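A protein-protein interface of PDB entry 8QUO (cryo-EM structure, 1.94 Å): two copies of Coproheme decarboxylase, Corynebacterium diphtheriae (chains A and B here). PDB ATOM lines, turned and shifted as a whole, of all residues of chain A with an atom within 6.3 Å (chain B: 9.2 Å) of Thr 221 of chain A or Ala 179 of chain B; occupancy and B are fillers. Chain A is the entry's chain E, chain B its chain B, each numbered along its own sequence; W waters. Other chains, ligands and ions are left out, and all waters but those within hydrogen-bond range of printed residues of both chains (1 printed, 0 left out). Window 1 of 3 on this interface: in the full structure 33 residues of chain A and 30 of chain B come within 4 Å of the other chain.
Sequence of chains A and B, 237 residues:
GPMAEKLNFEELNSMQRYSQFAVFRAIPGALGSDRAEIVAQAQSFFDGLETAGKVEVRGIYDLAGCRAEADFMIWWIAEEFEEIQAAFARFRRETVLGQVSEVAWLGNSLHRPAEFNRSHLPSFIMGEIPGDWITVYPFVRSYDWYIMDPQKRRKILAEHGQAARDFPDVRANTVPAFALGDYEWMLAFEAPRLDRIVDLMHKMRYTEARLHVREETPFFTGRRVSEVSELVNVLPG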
ATOM      1  N   ASP A  62       8.979  21.417  22.739  1.00  0.00           N
ATOM      2  CA  ASP A  62       7.765  22.156  23.054  1.00  0.00           C
ATOM      3  C   ASP A  62       6.564  21.236  22.861  1.00  0.00           C
ATOM      4  O   ASP A  62       6.287  20.798  21.740  1.00  0.00           O
ATOM      5  CB  ASP A  62       7.653  23.392  22.163  1.00  0.00           C
ATOM      6  CG  ASP A  62       6.414  24.217  22.451  1.00  0.00           C
ATOM      7  OD1 ASP A  62       5.756  23.983  23.486  1.00  0.00           O
ATOM      8  OD2 ASP A  62       6.095  25.105  21.635  1.00  0.00           O
ATOM      9  N   LEU A  63       5.853  20.951  23.949  1.00  0.00           N
ATOM     10  CA  LEU A  63       4.709  20.051  23.927  1.00  0.00           C
ATOM     11  C   LEU A  63       3.378  20.789  23.905  1.00  0.00           C
ATOM     12  O   LEU A  63       2.338  20.169  24.148  1.00  0.00           O
ATOM     13  CB  LEU A  63       4.753  19.108  25.131  1.00  0.00           C
ATOM     14  CG  LEU A  63       6.024  18.294  25.367  1.00  0.00           C
ATOM     15  CD1 LEU A  63       5.816  17.327  26.517  1.00  0.00           C
ATOM     16  CD2 LEU A  63       6.428  17.550  24.113  1.00  0.00           C
ATOM     17  N   ALA A  64       3.385  22.092  23.634  1.00  0.00           N
ATOM     18  CA  ALA A  64       2.151  22.864  23.638  1.00  0.00           C
ATOM     19  C   ALA A  64       1.182  22.333  22.589  1.00  0.00           C
ATOM     20  O   ALA A  64       1.558  22.102  21.438  1.00  0.00           O
ATOM     21  CB  ALA A  64       2.450  24.340  23.381  1.00  0.00           C
ATOM     22  N   GLY A  65      -0.069  22.140  22.994  1.00  0.00           N
ATOM     23  CA  GLY A  65      -1.097  21.654  22.102  1.00  0.00           C
ATOM     24  C   GLY A  65      -1.178  20.151  21.958  1.00  0.00           C
ATOM     25  O   GLY A  65      -2.087  19.662  21.277  1.00  0.00           O
ATOM     26  N   CYS A  66      -0.265  19.401  22.573  1.00  0.00           N
ATOM     27  CA  CYS A  66      -0.308  17.946  22.475  1.00  0.00           C
ATOM     28  C   CYS A  66      -1.345  17.359  23.426  1.00  0.00           C
ATOM     29  O   CYS A  66      -2.258  16.643  23.004  1.00  0.00           O
ATOM     30  CB  CYS A  66       1.075  17.355  22.759  1.00  0.00           C
ATOM     31  SG  CYS A  66       1.064  15.580  23.093  1.00  0.00           S
ATOM     32  N   TRP A 133      10.830  16.794  14.949  1.00  0.00           N
ATOM     33  CA  TRP A 133       9.632  16.381  15.665  1.00  0.00           C
ATOM     34  C   TRP A 133       9.888  15.059  16.369  1.00  0.00           C
ATOM     35  O   TRP A 133      10.576  14.185  15.832  1.00  0.00           O
ATOM     36  CB  TRP A 133       8.445  16.243  14.713  1.00  0.00           C
ATOM     37  CG  TRP A 133       7.912  17.556  14.262  1.00  0.00           C
ATOM     38  CD1 TRP A 133       8.299  18.264  13.166  1.00  0.00           C
ATOM     39  CD2 TRP A 133       6.900  18.331  14.906  1.00  0.00           C
ATOM     40  NE1 TRP A 133       7.585  19.432  13.083  1.00  0.00           N
ATOM     41  CE2 TRP A 133       6.718  19.497  14.141  1.00  0.00           C
ATOM     42  CE3 TRP A 133       6.126  18.151  16.055  1.00  0.00           C
ATOM     43  CZ2 TRP A 133       5.795  20.477  14.487  1.00  0.00           C
ATOM     44  CZ3 TRP A 133       5.212  19.124  16.396  1.00  0.00           C
ATOM     45  CH2 TRP A 133       5.054  20.272  15.616  1.00  0.00           C
ATOM     46  N   ILE A 134       9.336  14.914  17.572  1.00  0.00           N
ATOM     47  CA  ILE A 134       9.496  13.692  18.345  1.00  0.00           C
ATOM     48  C   ILE A 134       8.146  13.261  18.900  1.00  0.00           C
ATOM     49  O   ILE A 134       7.260  14.081  19.158  1.00  0.00           O
ATOM     50  CB  ILE A 134      10.523  13.855  19.490  1.00  0.00           C
ATOM     51  CG1 ILE A 134      11.102  12.496  19.887  1.00  0.00           C
ATOM     52  CG2 ILE A 134       9.887  14.519  20.698  1.00  0.00           C
ATOM     53  CD1 ILE A 134      12.116  12.568  21.001  1.00  0.00           C
ATOM     54  N   THR A 135       7.990  11.950  19.053  1.00  0.00           N
ATOM     55  CA  THR A 135       6.897  11.362  19.811  1.00  0.00           C
ATOM     56  C   THR A 135       7.491  10.371  20.802  1.00  0.00           C
ATOM     57  O   THR A 135       8.455   9.669  20.490  1.00  0.00           O
ATOM     58  CB  THR A 135       5.850  10.693  18.891  1.00  0.00           C
ATOM     59  OG1 THR A 135       4.584  10.645  19.561  1.00  0.00           O
ATOM     60  CG2 THR A 135       6.257   9.285  18.485  1.00  0.00           C
ATOM     61  N   VAL A 136       6.956  10.361  22.019  1.00  0.00           N
ATOM     62  CA  VAL A 136       7.503   9.552  23.102  1.00  0.00           C
ATOM     63  C   VAL A 136       6.349   8.896  23.841  1.00  0.00           C
ATOM     64  O   VAL A 136       5.350   9.554  24.149  1.00  0.00           O
ATOM     65  CB  VAL A 136       8.356  10.399  24.070  1.00  0.00           C
ATOM     66  CG1 VAL A 136       8.621   9.641  25.359  1.00  0.00           C
ATOM     67  CG2 VAL A 136       9.661  10.805  23.414  1.00  0.00           C
ATOM     68  N   LEU A 194       6.012  15.829  11.291  1.00  0.00           N
ATOM     69  CA  LEU A 194       5.079  15.156  12.189  1.00  0.00           C
ATOM     70  C   LEU A 194       4.167  14.199  11.430  1.00  0.00           C
ATOM     71  O   LEU A 194       3.815  13.127  11.943  1.00  0.00           O
ATOM     72  CB  LEU A 194       4.258  16.194  12.950  1.00  0.00           C
ATOM     73  CG  LEU A 194       3.265  15.671  13.985  1.00  0.00           C
ATOM     74  CD1 LEU A 194       3.949  14.696  14.920  1.00  0.00           C
ATOM     75  CD2 LEU A 194       2.658  16.826  14.756  1.00  0.00           C
ATOM     76  N   ILE A 197       5.497  10.763  11.277  1.00  0.00           N
ATOM     77  CA  ILE A 197       5.282   9.995  12.500  1.00  0.00           C
ATOM     78  C   ILE A 197       3.851   9.479  12.558  1.00  0.00           C
ATOM     79  O   ILE A 197       3.606   8.323  12.923  1.00  0.00           O
ATOM     80  CB  ILE A 197       5.624  10.843  13.739  1.00  0.00           C
ATOM     81  CG1 ILE A 197       7.114  11.167  13.775  1.00  0.00           C
ATOM     82  CG2 ILE A 197       5.222  10.120  15.010  1.00  0.00           C
ATOM     83  CD1 ILE A 197       7.499  12.135  14.869  1.00  0.00           C
ATOM     84  N   VAL A 198       2.885  10.328  12.201  1.00  0.00           N
ATOM     85  CA  VAL A 198       1.484   9.912  12.234  1.00  0.00           C
ATOM     86  C   VAL A 198       1.246   8.760  11.262  1.00  0.00           C
ATOM     87  O   VAL A 198       0.589   7.765  11.596  1.00  0.00           O
ATOM     88  CB  VAL A 198       0.561  11.106  11.932  1.00  0.00           C
ATOM     89  CG1 VAL A 198      -0.891  10.662  11.906  1.00  0.00           C
ATOM     90  CG2 VAL A 198       0.766  12.203  12.962  1.00  0.00           C
ATOM     91  N   MET A 201       2.834   5.530  12.582  1.00  0.00           N
ATOM     92  CA  MET A 201       2.050   4.946  13.666  1.00  0.00           C
ATOM     93  C   MET A 201       0.778   4.299  13.137  1.00  0.00           C
ATOM     94  O   MET A 201       0.364   3.240  13.624  1.00  0.00           O
ATOM     95  CB  MET A 201       1.722   6.009  14.713  1.00  0.00           C
ATOM     96  CG  MET A 201       1.272   5.439  16.047  1.00  0.00           C
ATOM     97  SD  MET A 201       2.621   4.913  17.125  1.00  0.00           S
ATOM     98  CE  MET A 201       3.968   5.942  16.546  1.00  0.00           C
ATOM     99  N   PHE A 219       0.972   9.526  25.506  1.00  0.00           N
ATOM    100  CA  PHE A 219       1.796   9.985  24.398  1.00  0.00           C
ATOM    101  C   PHE A 219       2.241  11.421  24.639  1.00  0.00           C
ATOM    102  O   PHE A 219       1.512  12.225  25.224  1.00  0.00           O
ATOM    103  CB  PHE A 219       1.029   9.913  23.078  1.00  0.00           C
ATOM    104  CG  PHE A 219       1.205   8.624  22.333  1.00  0.00           C
ATOM    105  CD1 PHE A 219       0.615   7.458  22.787  1.00  0.00           C
ATOM    106  CD2 PHE A 219       1.946   8.583  21.167  1.00  0.00           C
ATOM    107  CE1 PHE A 219       0.770   6.275  22.095  1.00  0.00           C
ATOM    108  CE2 PHE A 219       2.102   7.403  20.472  1.00  0.00           C
ATOM    109  CZ  PHE A 219       1.515   6.247  20.938  1.00  0.00           C
ATOM    110  N   PHE A 220       3.445  11.741  24.174  1.00  0.00           N
ATOM    111  CA  PHE A 220       3.973  13.101  24.244  1.00  0.00           C
ATOM    112  C   PHE A 220       4.591  13.433  22.896  1.00  0.00           C
ATOM    113  O   PHE A 220       5.623  12.866  22.528  1.00  0.00           O
ATOM    114  CB  PHE A 220       4.995  13.240  25.369  1.00  0.00           C
ATOM    115  CG  PHE A 220       4.433  12.966  26.731  1.00  0.00           C
ATOM    116  CD1 PHE A 220       3.762  13.953  27.430  1.00  0.00           C
ATOM    117  CD2 PHE A 220       4.570  11.719  27.310  1.00  0.00           C
ATOM    118  CE1 PHE A 220       3.241  13.699  28.681  1.00  0.00           C
ATOM    119  CE2 PHE A 220       4.051  11.462  28.559  1.00  0.00           C
ATOM    120  CZ  PHE A 220       3.386  12.453  29.246  1.00  0.00           C
ATOM    121  N   THR A 221       3.959  14.339  22.160  1.00  0.00           N
ATOM    122  CA  THR A 221       4.413  14.747  20.840  1.00  0.00           C
ATOM    123  C   THR A 221       4.887  16.191  20.907  1.00  0.00           C
ATOM    124  O   THR A 221       4.170  17.057  21.417  1.00  0.00           O
ATOM    125  CB  THR A 221       3.293  14.602  19.807  1.00  0.00           C
ATOM    126  OG1 THR A 221       2.961  13.217  19.654  1.00  0.00           O
ATOM    127  CG2 THR A 221       3.727  15.162  18.470  1.00  0.00           C
ATOM    128  N   GLY A 222       6.089  16.448  20.394  1.00  0.00           N
ATOM    129  CA  GLY A 222       6.672  17.765  20.544  1.00  0.00           C
ATOM    130  C   GLY A 222       7.605  18.149  19.416  1.00  0.00           C
ATOM    131  O   GLY A 222       8.030  17.320  18.608  1.00  0.00           O
ATOM    132  N   ARG A 223       7.914  19.441  19.378  1.00  0.00           N
ATOM    133  CA  ARG A 223       8.807  20.023  18.386  1.00  0.00           C
ATOM    134  C   ARG A 223      10.097  20.455  19.067  1.00  0.00           C
ATOM    135  O   ARG A 223      10.061  21.102  20.118  1.00  0.00           O
ATOM    136  CB  ARG A 223       8.149  21.219  17.694  1.00  0.00           C
ATOM    137  CG  ARG A 223       8.946  21.778  16.531  1.00  0.00           C
ATOM    138  CD  ARG A 223       8.315  23.044  15.988  1.00  0.00           C
ATOM    139  NE  ARG A 223       8.081  24.028  17.038  1.00  0.00           N
ATOM    140  CZ  ARG A 223       8.939  24.981  17.374  1.00  0.00           C
ATOM    141  NH1 ARG A 223      10.104  25.111  16.761  1.00  0.00           N
ATOM    142  NH2 ARG A 223       8.620  25.824  18.352  1.00  0.00           N
ATOM    143  N   TYR B  18      -4.185  19.713   9.704  1.00  0.00           N
ATOM    144  CA  TYR B  18      -4.271  19.380  11.117  1.00  0.00           C
ATOM    145  C   TYR B  18      -5.478  20.072  11.731  1.00  0.00           C
ATOM    146  O   TYR B  18      -5.764  21.234  11.429  1.00  0.00           O
ATOM    147  CB  TYR B  18      -3.001  19.801  11.858  1.00  0.00           C
ATOM    148  CG  TYR B  18      -1.775  18.993  11.511  1.00  0.00           C
ATOM    149  CD1 TYR B  18      -0.947  19.368  10.467  1.00  0.00           C
ATOM    150  CD2 TYR B  18      -1.440  17.861  12.239  1.00  0.00           C
ATOM    151  CE1 TYR B  18       0.178  18.637  10.151  1.00  0.00           C
ATOM    152  CE2 TYR B  18      -0.318  17.124  11.931  1.00  0.00           C
ATOM    153  CZ  TYR B  18       0.487  17.515  10.886  1.00  0.00           C
ATOM    154  OH  TYR B  18       1.606  16.783  10.575  1.00  0.00           O
ATOM    155  N   PHE B  81       1.026  21.918  11.933  1.00  0.00           N
ATOM    156  CA  PHE B  81       0.751  21.806  13.359  1.00  0.00           C
ATOM    157  C   PHE B  81       1.489  22.859  14.175  1.00  0.00           C
ATOM    158  O   PHE B  81       1.055  23.176  15.287  1.00  0.00           O
ATOM    159  CB  PHE B  81       1.112  20.409  13.862  1.00  0.00           C
ATOM    160  CG  PHE B  81       0.559  20.097  15.221  1.00  0.00           C
ATOM    161  CD1 PHE B  81      -0.806  19.984  15.416  1.00  0.00           C
ATOM    162  CD2 PHE B  81       1.403  19.919  16.302  1.00  0.00           C
ATOM    163  CE1 PHE B  81      -1.319  19.699  16.664  1.00  0.00           C
ATOM    164  CE2 PHE B  81       0.894  19.633  17.552  1.00  0.00           C
ATOM    165  CZ  PHE B  81      -0.468  19.523  17.734  1.00  0.00           C
ATOM    166  N   GLN B  85       0.002  25.033  17.270  1.00  0.00           N
ATOM    167  CA  GLN B  85       0.722  25.191  18.531  1.00  0.00           C
ATOM    168  C   GLN B  85       0.874  26.662  18.893  1.00  0.00           C
ATOM    169  O   GLN B  85       0.649  27.061  20.042  1.00  0.00           O
ATOM    170  CB  GLN B  85       2.097  24.531  18.435  1.00  0.00           C
ATOM    171  CG  GLN B  85       2.086  23.021  18.444  1.00  0.00           C
ATOM    172  CD  GLN B  85       3.460  22.444  18.707  1.00  0.00           C
ATOM    173  OE1 GLN B  85       4.376  22.606  17.901  1.00  0.00           O
ATOM    174  NE2 GLN B  85       3.616  21.772  19.839  1.00  0.00           N
ATOM    175  N   LEU B 106      -7.374  17.961  24.969  1.00  0.00           N
ATOM    176  CA  LEU B 106      -6.966  18.360  23.629  1.00  0.00           C
ATOM    177  C   LEU B 106      -7.158  17.184  22.684  1.00  0.00           C
ATOM    178  O   LEU B 106      -6.627  16.097  22.931  1.00  0.00           O
ATOM    179  CB  LEU B 106      -5.509  18.829  23.609  1.00  0.00           C
ATOM    180  CG  LEU B 106      -5.200  20.129  24.352  1.00  0.00           C
ATOM    181  CD1 LEU B 106      -3.705  20.350  24.446  1.00  0.00           C
ATOM    182  CD2 LEU B 106      -5.867  21.300  23.661  1.00  0.00           C
ATOM    183  N   ASN B 108      -6.331  16.143  18.935  1.00  0.00           N
ATOM    184  CA  ASN B 108      -5.571  16.469  17.740  1.00  0.00           C
ATOM    185  C   ASN B 108      -5.768  15.393  16.683  1.00  0.00           C
ATOM    186  O   ASN B 108      -5.963  14.217  17.000  1.00  0.00           O
ATOM    187  CB  ASN B 108      -4.081  16.614  18.059  1.00  0.00           C
ATOM    188  CG  ASN B 108      -3.812  17.661  19.114  1.00  0.00           C
ATOM    189  OD1 ASN B 108      -4.259  18.799  19.001  1.00  0.00           O
ATOM    190  ND2 ASN B 108      -3.076  17.282  20.149  1.00  0.00           N
ATOM    191  N   SER B 109      -5.714  15.807  15.420  1.00  0.00           N
ATOM    192  CA  SER B 109      -5.915  14.874  14.323  1.00  0.00           C
ATOM    193  C   SER B 109      -5.300  15.448  13.055  1.00  0.00           C
ATOM    194  O   SER B 109      -5.122  16.661  12.922  1.00  0.00           O
ATOM    195  CB  SER B 109      -7.401  14.572  14.121  1.00  0.00           C
ATOM    196  OG  SER B 109      -8.134  15.758  13.882  1.00  0.00           O
ATOM    197  N   LEU B 110      -4.977  14.552  12.127  1.00  0.00           N
ATOM    198  CA  LEU B 110      -4.395  14.908  10.839  1.00  0.00           C
ATOM    199  C   LEU B 110      -5.210  14.250   9.739  1.00  0.00           C
ATOM    200  O   LEU B 110      -5.433  13.036   9.774  1.00  0.00           O
ATOM    201  CB  LEU B 110      -2.931  14.469  10.752  1.00  0.00           C
ATOM    202  CG  LEU B 110      -2.275  14.550   9.374  1.00  0.00           C
ATOM    203  CD1 LEU B 110      -2.186  15.991   8.903  1.00  0.00           C
ATOM    204  CD2 LEU B 110      -0.903  13.910   9.411  1.00  0.00           C
ATOM    205  N   PRO B 176      -7.841  10.600  11.392  1.00  0.00           N
ATOM    206  CA  PRO B 176      -6.816   9.844  12.123  1.00  0.00           C
ATOM    207  C   PRO B 176      -6.142  10.701  13.185  1.00  0.00           C
ATOM    208  O   PRO B 176      -5.907  11.894  12.990  1.00  0.00           O
ATOM    209  CB  PRO B 176      -5.832   9.428  11.026  1.00  0.00           C
ATOM    210  CG  PRO B 176      -6.631   9.454   9.775  1.00  0.00           C
ATOM    211  CD  PRO B 176      -7.613  10.569   9.937  1.00  0.00           C
ATOM    212  N   ALA B 177      -5.825  10.073  14.320  1.00  0.00           N
ATOM    213  CA  ALA B 177      -5.227  10.774  15.451  1.00  0.00           C
ATOM    214  C   ALA B 177      -4.023  10.031  16.018  1.00  0.00           C
ATOM    215  O   ALA B 177      -3.646  10.268  17.169  1.00  0.00           O
ATOM    216  CB  ALA B 177      -6.265  11.006  16.551  1.00  0.00           C
ATOM    217  N   PHE B 178      -3.415   9.143  15.236  1.00  0.00           N
ATOM    218  CA  PHE B 178      -2.275   8.374  15.719  1.00  0.00           C
ATOM    219  C   PHE B 178      -1.092   9.288  16.023  1.00  0.00           C
ATOM    220  O   PHE B 178      -0.801  10.226  15.276  1.00  0.00           O
ATOM    221  CB  PHE B 178      -1.870   7.323  14.685  1.00  0.00           C
ATOM    222  CG  PHE B 178      -2.996   6.431  14.251  1.00  0.00           C
ATOM    223  CD1 PHE B 178      -3.799   6.778  13.178  1.00  0.00           C
ATOM    224  CD2 PHE B 178      -3.247   5.242  14.910  1.00  0.00           C
ATOM    225  CE1 PHE B 178      -4.833   5.959  12.777  1.00  0.00           C
ATOM    226  CE2 PHE B 178      -4.277   4.420  14.512  1.00  0.00           C
ATOM    227  CZ  PHE B 178      -5.071   4.778  13.445  1.00  0.00           C
ATOM    228  N   ALA B 179      -0.419   9.002  17.144  1.00  0.00           N
ATOM    229  CA  ALA B 179       0.781   9.691  17.618  1.00  0.00           C
ATOM    230  C   ALA B 179       0.559  11.159  17.968  1.00  0.00           C
ATOM    231  O   ALA B 179       1.515  11.858  18.321  1.00  0.00           O
ATOM    232  CB  ALA B 179       1.914   9.587  16.593  1.00  0.00           C
ATOM    233  N   LEU B 180      -0.678  11.643  17.883  1.00  0.00           N
ATOM    234  CA  LEU B 180      -1.012  12.995  18.310  1.00  0.00           C
ATOM    235  C   LEU B 180      -1.692  13.012  19.671  1.00  0.00           C
ATOM    236  O   LEU B 180      -2.274  14.031  20.056  1.00  0.00           O
ATOM    237  CB  LEU B 180      -1.897  13.679  17.269  1.00  0.00           C
ATOM    238  CG  LEU B 180      -1.320  13.731  15.855  1.00  0.00           C
ATOM    239  CD1 LEU B 180      -2.329  14.302  14.880  1.00  0.00           C
ATOM    240  CD2 LEU B 180      -0.039  14.544  15.836  1.00  0.00           C
ATOM    241  N   GLY B 181      -1.632  11.906  20.398  1.00  0.00           N
ATOM    242  CA  GLY B 181      -2.321  11.776  21.665  1.00  0.00           C
ATOM    243  C   GLY B 181      -2.427  10.308  22.038  1.00  0.00           C
ATOM    244  O   GLY B 181      -1.704   9.468  21.510  1.00  0.00           O
ATOM    245  N   ASP B 182      -3.358  10.026  22.942  1.00  0.00           N
ATOM    246  CA  ASP B 182      -3.561   8.678  23.450  1.00  0.00           C
ATOM    247  C   ASP B 182      -4.542   7.870  22.612  1.00  0.00           C
ATOM    248  O   ASP B 182      -4.877   6.743  22.990  1.00  0.00           O
ATOM    249  CB  ASP B 182      -4.050   8.732  24.899  1.00  0.00           C
ATOM    250  CG  ASP B 182      -2.995   9.251  25.850  1.00  0.00           C
ATOM    251  OD1 ASP B 182      -1.825   9.367  25.434  1.00  0.00           O
ATOM    252  OD2 ASP B 182      -3.336   9.541  27.015  1.00  0.00           O
ATOM    253  N   TYR B 183      -5.005   8.408  21.489  1.00  0.00           N
ATOM    254  CA  TYR B 183      -6.116   7.831  20.750  1.00  0.00           C
ATOM    255  C   TYR B 183      -5.724   7.561  19.303  1.00  0.00           C
ATOM    256  O   TYR B 183      -4.656   7.956  18.833  1.00  0.00           O
ATOM    257  CB  TYR B 183      -7.333   8.757  20.810  1.00  0.00           C
ATOM    258  CG  TYR B 183      -7.513   9.401  22.162  1.00  0.00           C
ATOM    259  CD1 TYR B 183      -7.995   8.673  23.240  1.00  0.00           C
ATOM    260  CD2 TYR B 183      -7.198  10.737  22.363  1.00  0.00           C
ATOM    261  CE1 TYR B 183      -8.161   9.257  24.477  1.00  0.00           C
ATOM    262  CE2 TYR B 183      -7.360  11.329  23.597  1.00  0.00           C
ATOM    263  CZ  TYR B 183      -7.841  10.585  24.650  1.00  0.00           C
ATOM    264  OH  TYR B 183      -8.005  11.169  25.883  1.00  0.00           O
ATOM    265  N   GLU B 184      -6.620   6.870  18.598  1.00  0.00           N
ATOM    266  CA  GLU B 184      -6.407   6.503  17.205  1.00  0.00           C
ATOM    267  C   GLU B 184      -7.213   7.346  16.230  1.00  0.00           C
ATOM    268  O   GLU B 184      -6.732   7.624  15.127  1.00  0.00           O
ATOM    269  CB  GLU B 184      -6.752   5.026  16.990  1.00  0.00           C
ATOM    270  CG  GLU B 184      -5.878   4.068  17.775  1.00  0.00           C
ATOM    271  CD  GLU B 184      -6.260   2.620  17.558  1.00  0.00           C
ATOM    272  OE1 GLU B 184      -7.352   2.369  17.009  1.00  0.00           O
ATOM    273  OE2 GLU B 184      -5.471   1.731  17.937  1.00  0.00           O
ATOM    274  N   TRP B 185      -8.423   7.754  16.602  1.00  0.00           N
ATOM    275  CA  TRP B 185      -9.265   8.561  15.734  1.00  0.00           C
ATOM    276  C   TRP B 185      -9.924   9.668  16.540  1.00  0.00           C
ATOM    277  O   TRP B 185     -10.121   9.544  17.749  1.00  0.00           O
ATOM    278  CB  TRP B 185     -10.346   7.718  15.044  1.00  0.00           C
ATOM    279  CG  TRP B 185      -9.807   6.600  14.215  1.00  0.00           C
ATOM    280  CD1 TRP B 185      -9.467   5.352  14.643  1.00  0.00           C
ATOM    281  CD2 TRP B 185      -9.548   6.626  12.806  1.00  0.00           C
ATOM    282  NE1 TRP B 185      -9.009   4.599  13.591  1.00  0.00           N
ATOM    283  CE2 TRP B 185      -9.050   5.358  12.451  1.00  0.00           C
ATOM    284  CE3 TRP B 185      -9.690   7.597  11.812  1.00  0.00           C
ATOM    285  CZ2 TRP B 185      -8.691   5.038  11.146  1.00  0.00           C
ATOM    286  CZ3 TRP B 185      -9.334   7.277  10.518  1.00  0.00           C
ATOM    287  CH2 TRP B 185      -8.841   6.008  10.196  1.00  0.00           C
HETATM  288  O   HOH W   1      -4.357  15.169  23.738  1.00  0.00           O
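The side-chain amide nitrogen (ND2) of Asn 108 of chain B lies within hydrogen-bond range of the backbone carbonyl oxygen (O) of Cys 66 of chain A, 3.0 Å away. OG1 of Thr 221 of chain A sits close to O of Ala 179 of chain B, at 2.4 Å. The side-chain carboxylate (OD1) of Asp 182 of chain B is in hydrogen-bond range of the backbone NH (N) of Phe 219 of chain A, 2.8 Å away. The backbone carbonyl oxygen (O) of Gly 65 of chain A lies within hydrogen-bond range of the side-chain amide nitrogen (ND2) of Asn 108 of chain B (2.8 Å). The side-chain amide nitrogen (NE2) of Gln 85 of chain B sits at hydrogen-bond distance from the backbone carbonyl oxygen (O) of Ala 64 of chain A, at 2.6 Å. NE2 of Gln 85 of chain B sits at hydrogen-bond distance from O of Asp 62 of chain A, 3.4 Å away.
The side-chain hydroxyl of Thr 135 of chain A lies within hydrogen-bond range of the side-chain hydroxyl of Thr 221 of chain A, at 3.0 Å. SG of Cys 66 of chain A is in hydrogen-bond range of N of Thr 221 of chain A (3.3 Å). The side-chain amide nitrogen (ND2) of Asn 108 of chain B sits at hydrogen-bond distance from the backbone carbonyl oxygen (O) of Leu 180 of chain B (3.3 Å). The backbone NH (N) of Asp 62 of chain A lies within hydrogen-bond range of the backbone carbonyl oxygen (O) of Arg 223 of chain A. N of Ala 64 of chain A sits at hydrogen-bond distance from OD1 of Asp 62 of chain A.
Among the printed residues, merely in contact across the chains: Phe 219 of chain A with Gly 181 of chain B (3.1 Å), Trp 133 of chain A with Gln 85 of chain B (3.3 Å), Val 198 of chain A with Phe 178 of chain B (3.4 Å), Thr 135 of chain A with Ala 179 of chain B (3.5 Å), Gly 65 of chain A with Leu 106 of chain B (3.6 Å), Leu 194 of chain A with Tyr 18 of chain B (3.6 Å), Leu 194 of chain A with Phe 81 of chain B (3.7 Å), Leu 194 of chain A with Leu 180 of chain B (3.7 Å), Ile 197 of chain A with Ala 179 of chain B (3.7 Å), Trp 133 of chain A with Phe 81 of chain B (3.7 Å), Val 198 of chain A with Leu 180 of chain B (3.8 Å), Met 201 of chain A with Phe 178 of chain B (3.8 Å), Phe 219 of chain A with Ala 179 of chain B (3.9 Å), Gly 65 of chain A with Phe 81 of chain B (3.9 Å), Cys 66 of chain A with Leu 180 of chain B (3.9 Å) and Cys 66 of chain A with Leu 106 of chain B (3.9 Å).
Thr 221 of chain A touches just one residue of chain B: Ala 179 (2.4 Å). Of chain A, only Thr 135 (3.5 Å), Ile 197 (3.7 Å), Phe 219 (3.9 Å) and Thr 221 (2.4 Å) come within 4 Å of Ala 179 of chain B. No residue of chain B comes within 4 Å of Gly 222 of chain A. Of the printed residues of chain A, Gly 181 of chain B touches Phe 219 (3.1 Å). Of the printed residues of chain A, Phe 178 of chain B touches Val 198 and Met 201. Of the printed residues of chain B, Leu 194 of chain A touches Tyr 18, Phe 81 and Leu 180. Of the printed residues of chain B, Cys 66 of chain A touches Leu 106 (3.9 Å), Asn 108 (3.0 Å) and Leu 180 (3.9 Å). Printed residues of chain B within 4 Å of Ala 64 of chain A: Gln 85 (2.6 Å). Leu 110 of chain B touches none of the printed residues of chain A. Ser 109 of chain B touches none of the printed residues of chain A. The nearest printed residue of chain A that does not touch Leu 180 of chain B is Thr 221 of chain A (4.2 Å).
Of the 17 printed residues of chain B, 10 touch a printed residue of chain A. Hydrophobic or aromatic side chains of chain B that line the printed part of chain A: Tyr 18, Phe 81, Leu 106, Phe 178, Ala 179 and Leu 180. Along chain B the printed residues that touch a printed residue of chain A span positions 18 to 182. Along chain A the printed residues that touch a printed residue of chain B span positions 62 to 221.
No position is printed for both chains.
Water W1 lies within hydrogen-bond range of the backbone carbonyl oxygen (O) of Leu 106 of chain B (2.6 Å) and the backbone carbonyl oxygen (O) of Cys 66 of chain A (2.7 Å).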
